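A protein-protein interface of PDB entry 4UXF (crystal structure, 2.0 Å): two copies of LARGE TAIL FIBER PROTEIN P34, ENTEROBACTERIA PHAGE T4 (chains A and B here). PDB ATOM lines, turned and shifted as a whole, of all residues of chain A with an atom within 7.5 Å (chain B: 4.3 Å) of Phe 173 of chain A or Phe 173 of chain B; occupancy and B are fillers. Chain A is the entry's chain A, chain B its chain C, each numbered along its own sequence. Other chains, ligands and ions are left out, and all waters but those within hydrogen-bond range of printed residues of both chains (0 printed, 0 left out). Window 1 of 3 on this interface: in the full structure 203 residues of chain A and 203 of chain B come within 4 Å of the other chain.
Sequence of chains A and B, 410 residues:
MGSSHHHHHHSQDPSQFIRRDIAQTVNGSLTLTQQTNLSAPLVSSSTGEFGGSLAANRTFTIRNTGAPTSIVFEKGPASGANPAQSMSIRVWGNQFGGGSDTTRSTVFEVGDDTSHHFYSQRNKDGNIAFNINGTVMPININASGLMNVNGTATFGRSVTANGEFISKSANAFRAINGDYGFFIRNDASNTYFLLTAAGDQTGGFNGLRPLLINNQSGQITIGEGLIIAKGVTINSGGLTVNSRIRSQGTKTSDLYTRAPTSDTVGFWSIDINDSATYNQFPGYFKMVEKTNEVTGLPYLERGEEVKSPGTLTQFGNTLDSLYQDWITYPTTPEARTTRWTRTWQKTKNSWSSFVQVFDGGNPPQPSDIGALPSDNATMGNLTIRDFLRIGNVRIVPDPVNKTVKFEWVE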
ATOM      1  N   GLU A 164      20.497  11.031 -19.115  1.00  0.00           N
ATOM      2  CA  GLU A 164      19.912  10.071 -20.024  1.00  0.00           C
ATOM      3  C   GLU A 164      20.830   9.753 -21.198  1.00  0.00           C
ATOM      4  O   GLU A 164      21.556  10.641 -21.691  1.00  0.00           O
ATOM      5  CB  GLU A 164      18.633  10.718 -20.561  1.00  0.00           C
ATOM      6  CG  GLU A 164      17.705   9.819 -21.358  1.00  0.00           C
ATOM      7  CD  GLU A 164      16.384  10.525 -21.692  1.00  0.00           C
ATOM      8  OE1 GLU A 164      16.377  11.784 -21.801  1.00  0.00           O
ATOM      9  OE2 GLU A 164      15.358   9.804 -21.859  1.00  0.00           O
ATOM     10  N   PHE A 165      20.773   8.513 -21.679  1.00  0.00           N
ATOM     11  CA  PHE A 165      21.386   8.127 -22.941  1.00  0.00           C
ATOM     12  C   PHE A 165      20.321   8.250 -24.033  1.00  0.00           C
ATOM     13  O   PHE A 165      19.249   7.652 -23.930  1.00  0.00           O
ATOM     14  CB  PHE A 165      21.877   6.693 -22.916  1.00  0.00           C
ATOM     15  CG  PHE A 165      23.037   6.460 -22.008  1.00  0.00           C
ATOM     16  CD1 PHE A 165      24.332   6.604 -22.468  1.00  0.00           C
ATOM     17  CD2 PHE A 165      22.828   6.084 -20.698  1.00  0.00           C
ATOM     18  CE1 PHE A 165      25.414   6.383 -21.629  1.00  0.00           C
ATOM     19  CE2 PHE A 165      23.892   5.847 -19.851  1.00  0.00           C
ATOM     20  CZ  PHE A 165      25.190   6.003 -20.325  1.00  0.00           C
ATOM     21  N   ILE A 166      20.605   9.005 -25.079  1.00  0.00           N
ATOM     22  CA  ILE A 166      19.655   9.178 -26.185  1.00  0.00           C
ATOM     23  C   ILE A 166      20.365   8.768 -27.482  1.00  0.00           C
ATOM     24  O   ILE A 166      21.461   9.250 -27.741  1.00  0.00           O
ATOM     25  CB  ILE A 166      19.206  10.643 -26.291  1.00  0.00           C
ATOM     26  CG1 ILE A 166      18.560  11.123 -24.994  1.00  0.00           C
ATOM     27  CG2 ILE A 166      18.264  10.839 -27.484  1.00  0.00           C
ATOM     28  CD1 ILE A 166      19.241  12.307 -24.350  1.00  0.00           C
ATOM     29  N   SER A 167      19.760   7.873 -28.270  1.00  0.00           N
ATOM     30  CA  SER A 167      20.207   7.558 -29.621  1.00  0.00           C
ATOM     31  C   SER A 167      19.224   8.119 -30.641  1.00  0.00           C
ATOM     32  O   SER A 167      18.001   8.000 -30.448  1.00  0.00           O
ATOM     33  CB  SER A 167      20.309   6.053 -29.828  1.00  0.00           C
ATOM     34  OG  SER A 167      20.753   5.782 -31.168  1.00  0.00           O
ATOM     35  N   LYS A 168      19.736   8.705 -31.720  1.00  0.00           N
ATOM     36  CA  LYS A 168      18.926   9.085 -32.889  1.00  0.00           C
ATOM     37  C   LYS A 168      18.981   8.057 -34.019  1.00  0.00           C
ATOM     38  O   LYS A 168      18.493   8.312 -35.115  1.00  0.00           O
ATOM     39  CB  LYS A 168      19.400  10.420 -33.443  1.00  0.00           C
ATOM     40  CG  LYS A 168      19.542  11.547 -32.450  1.00  0.00           C
ATOM     41  CD  LYS A 168      18.236  11.939 -31.826  1.00  0.00           C
ATOM     42  CE  LYS A 168      18.393  13.183 -30.964  1.00  0.00           C
ATOM     43  NZ  LYS A 168      18.959  14.349 -31.697  1.00  0.00           N
ATOM     44  N   SER A 169      19.584   6.905 -33.756  1.00  0.00           N
ATOM     45  CA  SER A 169      19.687   5.817 -34.719  1.00  0.00           C
ATOM     46  C   SER A 169      18.474   4.924 -34.552  1.00  0.00           C
ATOM     47  O   SER A 169      18.085   4.635 -33.427  1.00  0.00           O
ATOM     48  CB  SER A 169      20.973   5.018 -34.444  1.00  0.00           C
ATOM     49  OG  SER A 169      21.131   3.885 -35.274  1.00  0.00           O
ATOM     50  N   ALA A 170      17.876   4.495 -35.660  1.00  0.00           N
ATOM     51  CA  ALA A 170      16.723   3.598 -35.607  1.00  0.00           C
ATOM     52  C   ALA A 170      17.091   2.383 -34.768  1.00  0.00           C
ATOM     53  O   ALA A 170      16.412   2.085 -33.829  1.00  0.00           O
ATOM     54  CB  ALA A 170      16.318   3.167 -36.999  1.00  0.00           C
ATOM     55  N   ASN A 171      18.212   1.730 -35.074  1.00  0.00           N
ATOM     56  CA  ASN A 171      18.796   0.744 -34.163  1.00  0.00           C
ATOM     57  C   ASN A 171      19.541   1.501 -33.084  1.00  0.00           C
ATOM     58  O   ASN A 171      20.585   2.088 -33.359  1.00  0.00           O
ATOM     59  CB  ASN A 171      19.730  -0.169 -34.905  1.00  0.00           C
ATOM     60  CG  ASN A 171      18.999  -1.093 -35.855  1.00  0.00           C
ATOM     61  OD1 ASN A 171      17.766  -1.213 -35.824  1.00  0.00           O
ATOM     62  ND2 ASN A 171      19.759  -1.752 -36.705  1.00  0.00           N
ATOM     63  N   ALA A 172      18.998   1.513 -31.869  1.00  0.00           N
ATOM     64  CA  ALA A 172      19.412   2.449 -30.817  1.00  0.00           C
ATOM     65  C   ALA A 172      20.313   1.838 -29.744  1.00  0.00           C
ATOM     66  O   ALA A 172      21.309   2.455 -29.341  1.00  0.00           O
ATOM     67  CB  ALA A 172      18.189   3.067 -30.194  1.00  0.00           C
ATOM     68  N   PHE A 173      19.922   0.669 -29.218  1.00  0.00           N
ATOM     69  CA  PHE A 173      20.616   0.052 -28.094  1.00  0.00           C
ATOM     70  C   PHE A 173      20.793  -1.419 -28.383  1.00  0.00           C
ATOM     71  O   PHE A 173      19.826  -2.122 -28.633  1.00  0.00           O
ATOM     72  CB  PHE A 173      19.894   0.271 -26.773  1.00  0.00           C
ATOM     73  CG  PHE A 173      19.684   1.711 -26.434  1.00  0.00           C
ATOM     74  CD1 PHE A 173      20.693   2.458 -25.826  1.00  0.00           C
ATOM     75  CD2 PHE A 173      18.496   2.347 -26.749  1.00  0.00           C
ATOM     76  CE1 PHE A 173      20.519   3.825 -25.554  1.00  0.00           C
ATOM     77  CE2 PHE A 173      18.310   3.684 -26.449  1.00  0.00           C
ATOM     78  CZ  PHE A 173      19.328   4.430 -25.870  1.00  0.00           C
ATOM     79  N   ARG A 174      22.034  -1.887 -28.343  1.00  0.00           N
ATOM     80  CA  ARG A 174      22.372  -3.264 -28.693  1.00  0.00           C
ATOM     81  C   ARG A 174      23.236  -3.917 -27.619  1.00  0.00           C
ATOM     82  O   ARG A 174      24.215  -3.315 -27.182  1.00  0.00           O
ATOM     83  CB  ARG A 174      23.109  -3.306 -30.032  1.00  0.00           C
ATOM     84  CG  ARG A 174      23.430  -4.728 -30.515  1.00  0.00           C
ATOM     85  CD  ARG A 174      24.026  -4.754 -31.881  1.00  0.00           C
ATOM     86  NE  ARG A 174      23.171  -4.124 -32.893  1.00  0.00           N
ATOM     87  CZ  ARG A 174      22.727  -4.684 -34.017  1.00  0.00           C
ATOM     88  NH1 ARG A 174      23.014  -5.954 -34.345  1.00  0.00           N
ATOM     89  NH2 ARG A 174      21.960  -3.962 -34.828  1.00  0.00           N
ATOM     90  N   ALA A 175      22.848  -5.138 -27.207  1.00  0.00           N
ATOM     91  CA  ALA A 175      23.586  -5.989 -26.265  1.00  0.00           C
ATOM     92  C   ALA A 175      24.070  -7.232 -27.023  1.00  0.00           C
ATOM     93  O   ALA A 175      23.240  -8.016 -27.522  1.00  0.00           O
ATOM     94  CB  ALA A 175      22.688  -6.383 -25.119  1.00  0.00           C
ATOM     95  N   ILE A 176      25.396  -7.374 -27.152  1.00  0.00           N
ATOM     96  CA  ILE A 176      26.044  -8.467 -27.878  1.00  0.00           C
ATOM     97  C   ILE A 176      26.671  -9.410 -26.861  1.00  0.00           C
ATOM     98  O   ILE A 176      27.428  -8.992 -25.957  1.00  0.00           O
ATOM     99  CB  ILE A 176      27.128  -7.945 -28.857  1.00  0.00           C
ATOM    100  CG1 ILE A 176      26.473  -7.234 -30.039  1.00  0.00           C
ATOM    101  CG2 ILE A 176      28.030  -9.083 -29.392  1.00  0.00           C
ATOM    102  CD1 ILE A 176      27.473  -6.482 -30.926  1.00  0.00           C
ATOM    103  N   PHE A 182      21.176  -8.581 -29.490  1.00  0.00           N
ATOM    104  CA  PHE A 182      19.807  -8.169 -29.153  1.00  0.00           C
ATOM    105  C   PHE A 182      19.762  -6.665 -29.243  1.00  0.00           C
ATOM    106  O   PHE A 182      20.679  -5.993 -28.729  1.00  0.00           O
ATOM    107  CB  PHE A 182      19.432  -8.594 -27.743  1.00  0.00           C
ATOM    108  CG  PHE A 182      18.186  -7.939 -27.235  1.00  0.00           C
ATOM    109  CD1 PHE A 182      16.936  -8.467 -27.554  1.00  0.00           C
ATOM    110  CD2 PHE A 182      18.258  -6.774 -26.483  1.00  0.00           C
ATOM    111  CE1 PHE A 182      15.778  -7.852 -27.116  1.00  0.00           C
ATOM    112  CE2 PHE A 182      17.112  -6.158 -26.031  1.00  0.00           C
ATOM    113  CZ  PHE A 182      15.870  -6.698 -26.343  1.00  0.00           C
ATOM    114  N   PHE A 183      18.730  -6.115 -29.894  1.00  0.00           N
ATOM    115  CA  PHE A 183      18.613  -4.693 -29.953  1.00  0.00           C
ATOM    116  C   PHE A 183      17.202  -4.122 -30.005  1.00  0.00           C
ATOM    117  O   PHE A 183      16.217  -4.771 -30.398  1.00  0.00           O
ATOM    118  CB  PHE A 183      19.490  -4.104 -31.078  1.00  0.00           C
ATOM    119  CG  PHE A 183      19.132  -4.565 -32.475  1.00  0.00           C
ATOM    120  CD1 PHE A 183      19.542  -5.813 -32.930  1.00  0.00           C
ATOM    121  CD2 PHE A 183      18.414  -3.733 -33.342  1.00  0.00           C
ATOM    122  CE1 PHE A 183      19.233  -6.256 -34.209  1.00  0.00           C
ATOM    123  CE2 PHE A 183      18.107  -4.168 -34.630  1.00  0.00           C
ATOM    124  CZ  PHE A 183      18.516  -5.423 -35.067  1.00  0.00           C
ATOM    125  N   ILE A 184      17.153  -2.869 -29.593  1.00  0.00           N
ATOM    126  CA  ILE A 184      15.965  -2.052 -29.606  1.00  0.00           C
ATOM    127  C   ILE A 184      16.046  -1.115 -30.795  1.00  0.00           C
ATOM    128  O   ILE A 184      17.024  -0.357 -30.931  1.00  0.00           O
ATOM    129  CB  ILE A 184      15.807  -1.255 -28.295  1.00  0.00           C
ATOM    130  CG1 ILE A 184      15.888  -2.187 -27.064  1.00  0.00           C
ATOM    131  CG2 ILE A 184      14.555  -0.405 -28.337  1.00  0.00           C
ATOM    132  CD1 ILE A 184      15.841  -1.443 -25.752  1.00  0.00           C
ATOM    133  N   ARG A 185      15.016  -1.182 -31.645  1.00  0.00           N
ATOM    134  CA  ARG A 185      14.931  -0.438 -32.888  1.00  0.00           C
ATOM    135  C   ARG A 185      13.611   0.333 -32.905  1.00  0.00           C
ATOM    136  O   ARG A 185      12.530  -0.279 -32.835  1.00  0.00           O
ATOM    137  CB  ARG A 185      14.985  -1.418 -34.063  1.00  0.00           C
ATOM    138  CG  ARG A 185      14.757  -0.789 -35.419  1.00  0.00           C
ATOM    139  CD  ARG A 185      14.727  -1.827 -36.534  1.00  0.00           C
ATOM    140  NE  ARG A 185      14.365  -1.167 -37.785  1.00  0.00           N
ATOM    141  CZ  ARG A 185      15.210  -0.505 -38.581  1.00  0.00           C
ATOM    142  NH1 ARG A 185      16.519  -0.432 -38.311  1.00  0.00           N
ATOM    143  NH2 ARG A 185      14.754   0.059 -39.692  1.00  0.00           N
ATOM    144  N   ASN A 186      13.701   1.659 -32.956  1.00  0.00           N
ATOM    145  CA  ASN A 186      12.553   2.525 -33.169  1.00  0.00           C
ATOM    146  C   ASN A 186      12.600   2.895 -34.618  1.00  0.00           C
ATOM    147  O   ASN A 186      13.483   3.652 -35.036  1.00  0.00           O
ATOM    148  CB  ASN A 186      12.644   3.773 -32.298  1.00  0.00           C
ATOM    149  CG  ASN A 186      11.489   4.746 -32.524  1.00  0.00           C
ATOM    150  OD1 ASN A 186      10.637   4.537 -33.356  1.00  0.00           O
ATOM    151  ND2 ASN A 186      11.484   5.815 -31.786  1.00  0.00           N
ATOM    152  N   TYR A 192      10.769  -2.040 -31.727  1.00  0.00           N
ATOM    153  CA  TYR A 192      10.928  -3.477 -31.756  1.00  0.00           C
ATOM    154  C   TYR A 192      12.069  -3.919 -30.861  1.00  0.00           C
ATOM    155  O   TYR A 192      13.084  -3.220 -30.763  1.00  0.00           O
ATOM    156  CB  TYR A 192      11.332  -3.934 -33.167  1.00  0.00           C
ATOM    157  CG  TYR A 192      10.349  -3.718 -34.255  1.00  0.00           C
ATOM    158  CD1 TYR A 192      10.208  -2.467 -34.846  1.00  0.00           C
ATOM    159  CD2 TYR A 192       9.594  -4.794 -34.761  1.00  0.00           C
ATOM    160  CE1 TYR A 192       9.307  -2.269 -35.903  1.00  0.00           C
ATOM    161  CE2 TYR A 192       8.687  -4.608 -35.799  1.00  0.00           C
ATOM    162  CZ  TYR A 192       8.547  -3.347 -36.366  1.00  0.00           C
ATOM    163  OH  TYR A 192       7.658  -3.154 -37.384  1.00  0.00           O
ATOM    164  N   LEU A 194      14.602  -6.875 -31.122  1.00  0.00           N
ATOM    165  CA  LEU A 194      15.002  -7.748 -32.206  1.00  0.00           C
ATOM    166  C   LEU A 194      16.293  -8.487 -31.915  1.00  0.00           C
ATOM    167  O   LEU A 194      17.021  -8.153 -30.989  1.00  0.00           O
ATOM    168  CB  LEU A 194      15.194  -6.918 -33.472  1.00  0.00           C
ATOM    169  CG  LEU A 194      13.935  -6.172 -33.920  1.00  0.00           C
ATOM    170  CD1 LEU A 194      14.267  -5.159 -34.994  1.00  0.00           C
ATOM    171  CD2 LEU A 194      12.918  -7.170 -34.451  1.00  0.00           C
ATOM    172  N   PHE B 165      24.149   2.611 -29.715  1.00  0.00           N
ATOM    173  CA  PHE B 165      24.917   2.247 -28.538  1.00  0.00           C
ATOM    174  C   PHE B 165      25.006   0.754 -28.497  1.00  0.00           C
ATOM    175  O   PHE B 165      23.981   0.080 -28.486  1.00  0.00           O
ATOM    176  CB  PHE B 165      24.261   2.692 -27.236  1.00  0.00           C
ATOM    177  CG  PHE B 165      24.274   4.172 -26.997  1.00  0.00           C
ATOM    178  CD1 PHE B 165      25.335   4.768 -26.341  1.00  0.00           C
ATOM    179  CD2 PHE B 165      23.193   4.942 -27.355  1.00  0.00           C
ATOM    180  CE1 PHE B 165      25.329   6.118 -26.076  1.00  0.00           C
ATOM    181  CE2 PHE B 165      23.161   6.284 -27.081  1.00  0.00           C
ATOM    182  CZ  PHE B 165      24.242   6.886 -26.475  1.00  0.00           C
ATOM    183  N   SER B 167      26.761  -2.485 -26.408  1.00  0.00           N
ATOM    184  CA  SER B 167      27.512  -3.065 -25.289  1.00  0.00           C
ATOM    185  C   SER B 167      27.892  -4.521 -25.588  1.00  0.00           C
ATOM    186  O   SER B 167      27.069  -5.297 -26.084  1.00  0.00           O
ATOM    187  CB  SER B 167      26.712  -3.022 -24.019  1.00  0.00           C
ATOM    188  OG  SER B 167      27.484  -3.531 -22.953  1.00  0.00           O
ATOM    189  N   ASN B 171      25.696  -7.944 -18.886  1.00  0.00           N
ATOM    190  CA  ASN B 171      24.896  -6.864 -18.348  1.00  0.00           C
ATOM    191  C   ASN B 171      25.219  -5.629 -19.159  1.00  0.00           C
ATOM    192  O   ASN B 171      26.335  -5.061 -19.062  1.00  0.00           O
ATOM    193  CB  ASN B 171      25.211  -6.637 -16.883  1.00  0.00           C
ATOM    194  CG  ASN B 171      24.791  -7.810 -16.009  1.00  0.00           C
ATOM    195  OD1 ASN B 171      24.092  -8.732 -16.463  1.00  0.00           O
ATOM    196  ND2 ASN B 171      25.219  -7.788 -14.754  1.00  0.00           N
ATOM    197  N   ALA B 172      24.245  -5.227 -19.975  1.00  0.00           N
ATOM    198  CA  ALA B 172      24.437  -4.294 -21.062  1.00  0.00           C
ATOM    199  C   ALA B 172      23.971  -2.851 -20.834  1.00  0.00           C
ATOM    200  O   ALA B 172      24.688  -1.892 -21.156  1.00  0.00           O
ATOM    201  CB  ALA B 172      23.775  -4.854 -22.315  1.00  0.00           C
ATOM    202  N   PHE B 173      22.749  -2.695 -20.349  1.00  0.00           N
ATOM    203  CA  PHE B 173      22.124  -1.391 -20.129  1.00  0.00           C
ATOM    204  C   PHE B 173      21.369  -1.447 -18.797  1.00  0.00           C
ATOM    205  O   PHE B 173      20.537  -2.338 -18.579  1.00  0.00           O
ATOM    206  CB  PHE B 173      21.155  -1.019 -21.259  1.00  0.00           C
ATOM    207  CG  PHE B 173      21.786  -1.020 -22.615  1.00  0.00           C
ATOM    208  CD1 PHE B 173      22.457   0.110 -23.087  1.00  0.00           C
ATOM    209  CD2 PHE B 173      21.742  -2.161 -23.420  1.00  0.00           C
ATOM    210  CE1 PHE B 173      23.076   0.104 -24.336  1.00  0.00           C
ATOM    211  CE2 PHE B 173      22.358  -2.171 -24.658  1.00  0.00           C
ATOM    212  CZ  PHE B 173      23.032  -1.046 -25.118  1.00  0.00           C
ATOM    213  N   ARG B 174      21.684  -0.516 -17.915  1.00  0.00           N
ATOM    214  CA  ARG B 174      21.170  -0.466 -16.568  1.00  0.00           C
ATOM    215  C   ARG B 174      20.661   0.933 -16.233  1.00  0.00           C
ATOM    216  O   ARG B 174      21.343   1.950 -16.509  1.00  0.00           O
ATOM    217  CB  ARG B 174      22.259  -0.854 -15.585  1.00  0.00           C
ATOM    218  CG  ARG B 174      21.843  -0.787 -14.118  1.00  0.00           C
ATOM    219  CD  ARG B 174      22.928  -1.303 -13.185  1.00  0.00           C
ATOM    220  NE  ARG B 174      23.400  -2.657 -13.499  1.00  0.00           N
ATOM    221  CZ  ARG B 174      23.430  -3.705 -12.673  1.00  0.00           C
ATOM    222  NH1 ARG B 174      22.983  -3.643 -11.403  1.00  0.00           N
ATOM    223  NH2 ARG B 174      23.919  -4.847 -13.128  1.00  0.00           N
ATOM    224  N   PHE B 182      17.559  -1.656 -12.599  1.00  0.00           N
ATOM    225  CA  PHE B 182      16.959  -2.448 -13.649  1.00  0.00           C
ATOM    226  C   PHE B 182      17.964  -2.583 -14.776  1.00  0.00           C
ATOM    227  O   PHE B 182      18.590  -1.600 -15.157  1.00  0.00           O
ATOM    228  CB  PHE B 182      15.714  -1.717 -14.184  1.00  0.00           C
ATOM    229  CG  PHE B 182      15.174  -2.328 -15.447  1.00  0.00           C
ATOM    230  CD1 PHE B 182      14.331  -3.441 -15.384  1.00  0.00           C
ATOM    231  CD2 PHE B 182      15.529  -1.818 -16.690  1.00  0.00           C
ATOM    232  CE1 PHE B 182      13.865  -4.028 -16.558  1.00  0.00           C
ATOM    233  CE2 PHE B 182      15.065  -2.392 -17.875  1.00  0.00           C
ATOM    234  CZ  PHE B 182      14.233  -3.509 -17.808  1.00  0.00           C
ATOM    235  N   PHE B 183      18.095  -3.771 -15.346  1.00  0.00           N
ATOM    236  CA  PHE B 183      19.036  -4.003 -16.412  1.00  0.00           C
ATOM    237  C   PHE B 183      18.668  -5.080 -17.396  1.00  0.00           C
ATOM    238  O   PHE B 183      17.950  -6.022 -17.080  1.00  0.00           O
ATOM    239  CB  PHE B 183      20.481  -4.210 -15.925  1.00  0.00           C
ATOM    240  CG  PHE B 183      20.699  -5.361 -14.989  1.00  0.00           C
ATOM    241  CD1 PHE B 183      20.333  -5.268 -13.651  1.00  0.00           C
ATOM    242  CD2 PHE B 183      21.349  -6.512 -15.429  1.00  0.00           C
ATOM    243  CE1 PHE B 183      20.572  -6.313 -12.766  1.00  0.00           C
ATOM    244  CE2 PHE B 183      21.589  -7.573 -14.565  1.00  0.00           C
ATOM    245  CZ  PHE B 183      21.207  -7.476 -13.225  1.00  0.00           C
ATOM    246  N   ILE B 184      19.172  -4.881 -18.611  1.00  0.00           N
ATOM    247  CA  ILE B 184      19.083  -5.823 -19.689  1.00  0.00           C
ATOM    248  C   ILE B 184      20.368  -6.615 -19.768  1.00  0.00           C
ATOM    249  O   ILE B 184      21.447  -6.017 -19.873  1.00  0.00           O
ATOM    250  CB  ILE B 184      18.865  -5.086 -21.016  1.00  0.00           C
ATOM    251  CG1 ILE B 184      17.562  -4.248 -20.909  1.00  0.00           C
ATOM    252  CG2 ILE B 184      18.833  -6.085 -22.172  1.00  0.00           C
ATOM    253  CD1 ILE B 184      17.272  -3.308 -22.060  1.00  0.00           C
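The backbone NH of Phe 165 of chain B is in hydrogen-bond range of the backbone carbonyl oxygen of Ala 172 of chain A (2.9 Å). The backbone NH (N) of Arg 174 of chain A is in hydrogen-bond range of the backbone carbonyl oxygen (O) of Phe 165 of chain B. O of Arg 174 of chain A is in hydrogen-bond range of N of Ser 167 of chain B, at 2.8 Å. N of Ile 176 of chain A is in hydrogen-bond range of O of Ser 167 of chain B, at 2.9 Å.
The backbone NH (N) of Ser 169 of chain A lies within hydrogen-bond range of the side-chain hydroxyl (OG) of Ser 167 of chain A (3.1 Å). The backbone NH (N) of Ala 172 of chain A is in hydrogen-bond range of the backbone carbonyl oxygen (O) of Ile 184 of chain A (2.9 Å). The backbone NH of Ile 184 of chain A sits at hydrogen-bond distance from the backbone carbonyl oxygen of Phe 173 of chain A, 2.9 Å away. The backbone NH (N) of Ala 175 of chain A lies within hydrogen-bond range of the backbone carbonyl oxygen (O) of Phe 182 of chain A. O of Ile 184 of chain B is in hydrogen-bond range of N of Ala 172 of chain B (2.9 Å). The backbone NH of Ile 184 of chain B lies within hydrogen-bond range of the backbone carbonyl oxygen of Phe 173 of chain B (2.9 Å).
Among the printed residues, pairs that only touch across the chains: Arg 174 of chain A with Phe 173 of chain B (3.3 Å), Ala 175 of chain A with Ala 172 of chain B (3.4 Å), Phe 173 of chain A with Phe 165 of chain B (3.4 Å), Ile 166 of chain A with Phe 165 of chain B (3.5 Å), Ala 175 of chain A with Ser 167 of chain B (3.6 Å), Phe 173 of chain A with Phe 173 of chain B (3.7 Å), Phe 165 of chain A with Phe 165 of chain B (3.8 Å), Ser 167 of chain A with Phe 165 of chain B (3.9 Å) and Ala 175 of chain A with Phe 173 of chain B (3.9 Å).
Printed residues of chain B within 4 Å of Phe 165 of chain A: Phe 165 (3.8 Å). Ala 170 of chain A touches none of the printed residues of chain B. Phe 173 of chain A touches just these residues of chain B: Phe 165 and Phe 173. Printed residues of chain B within 4 Å of Arg 174 of chain A: Phe 165, Ser 167 and Phe 173. Of the printed residues of chain B, Ala 175 of chain A touches Ser 167 (3.6 Å), Ala 172 (3.4 Å) and Phe 173 (3.9 Å). Phe 183 of chain A touches none of the printed residues of chain B. Of the printed residues of chain A, Phe 165 of chain B touches Phe 165 (3.8 Å), Ile 166 (3.5 Å), Ser 167 (3.9 Å), Ala 172 (2.9 Å), Phe 173 (3.4 Å) and Arg 174 (2.8 Å). Ala 172 of chain B touches just one residue of chain A: Ala 175.
Hydrophobic or aromatic side chains of chain B that line the printed part of chain A: Phe 165, Ala 172 and Phe 173. Along chain B the printed residues that touch a printed residue of chain A span positions 165 to 173. Hydrophobic or aromatic side chains of chain A that line the printed part of chain B: Phe 165, Phe 173, Ala 175 and Ile 176. Among the printed residues, no Asp or Glu carboxylate lies within 4 Å of a Lys or Arg side-chain nitrogen of the other chain.
Ala 172 of chain A touches Phe 165 of chain B, but with the chains exchanged Phe 165 of chain A does not touch Ala 172 of chain B (7.9 Å). Phe 173 of chain A touches its own counterpart, Phe 173 of chain B. Arg 174 of chain A touches Phe 165 of chain B, but with the chains exchanged Phe 165 of chain A does not touch Arg 174 of chain B (5.7 Å). Arg 174 of chain A touches Phe 173 of chain B, but with the chains exchanged Phe 173 of chain A does not touch Arg 174 of chain B (8.5 Å). Positions printed for both chains: 165, 167, 171, 172, 173, 174, 182, 183 and 184. Of the 13 pairs that touch across the chains among the printed residues, 2 have their exchanged pair printed and touching as well.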
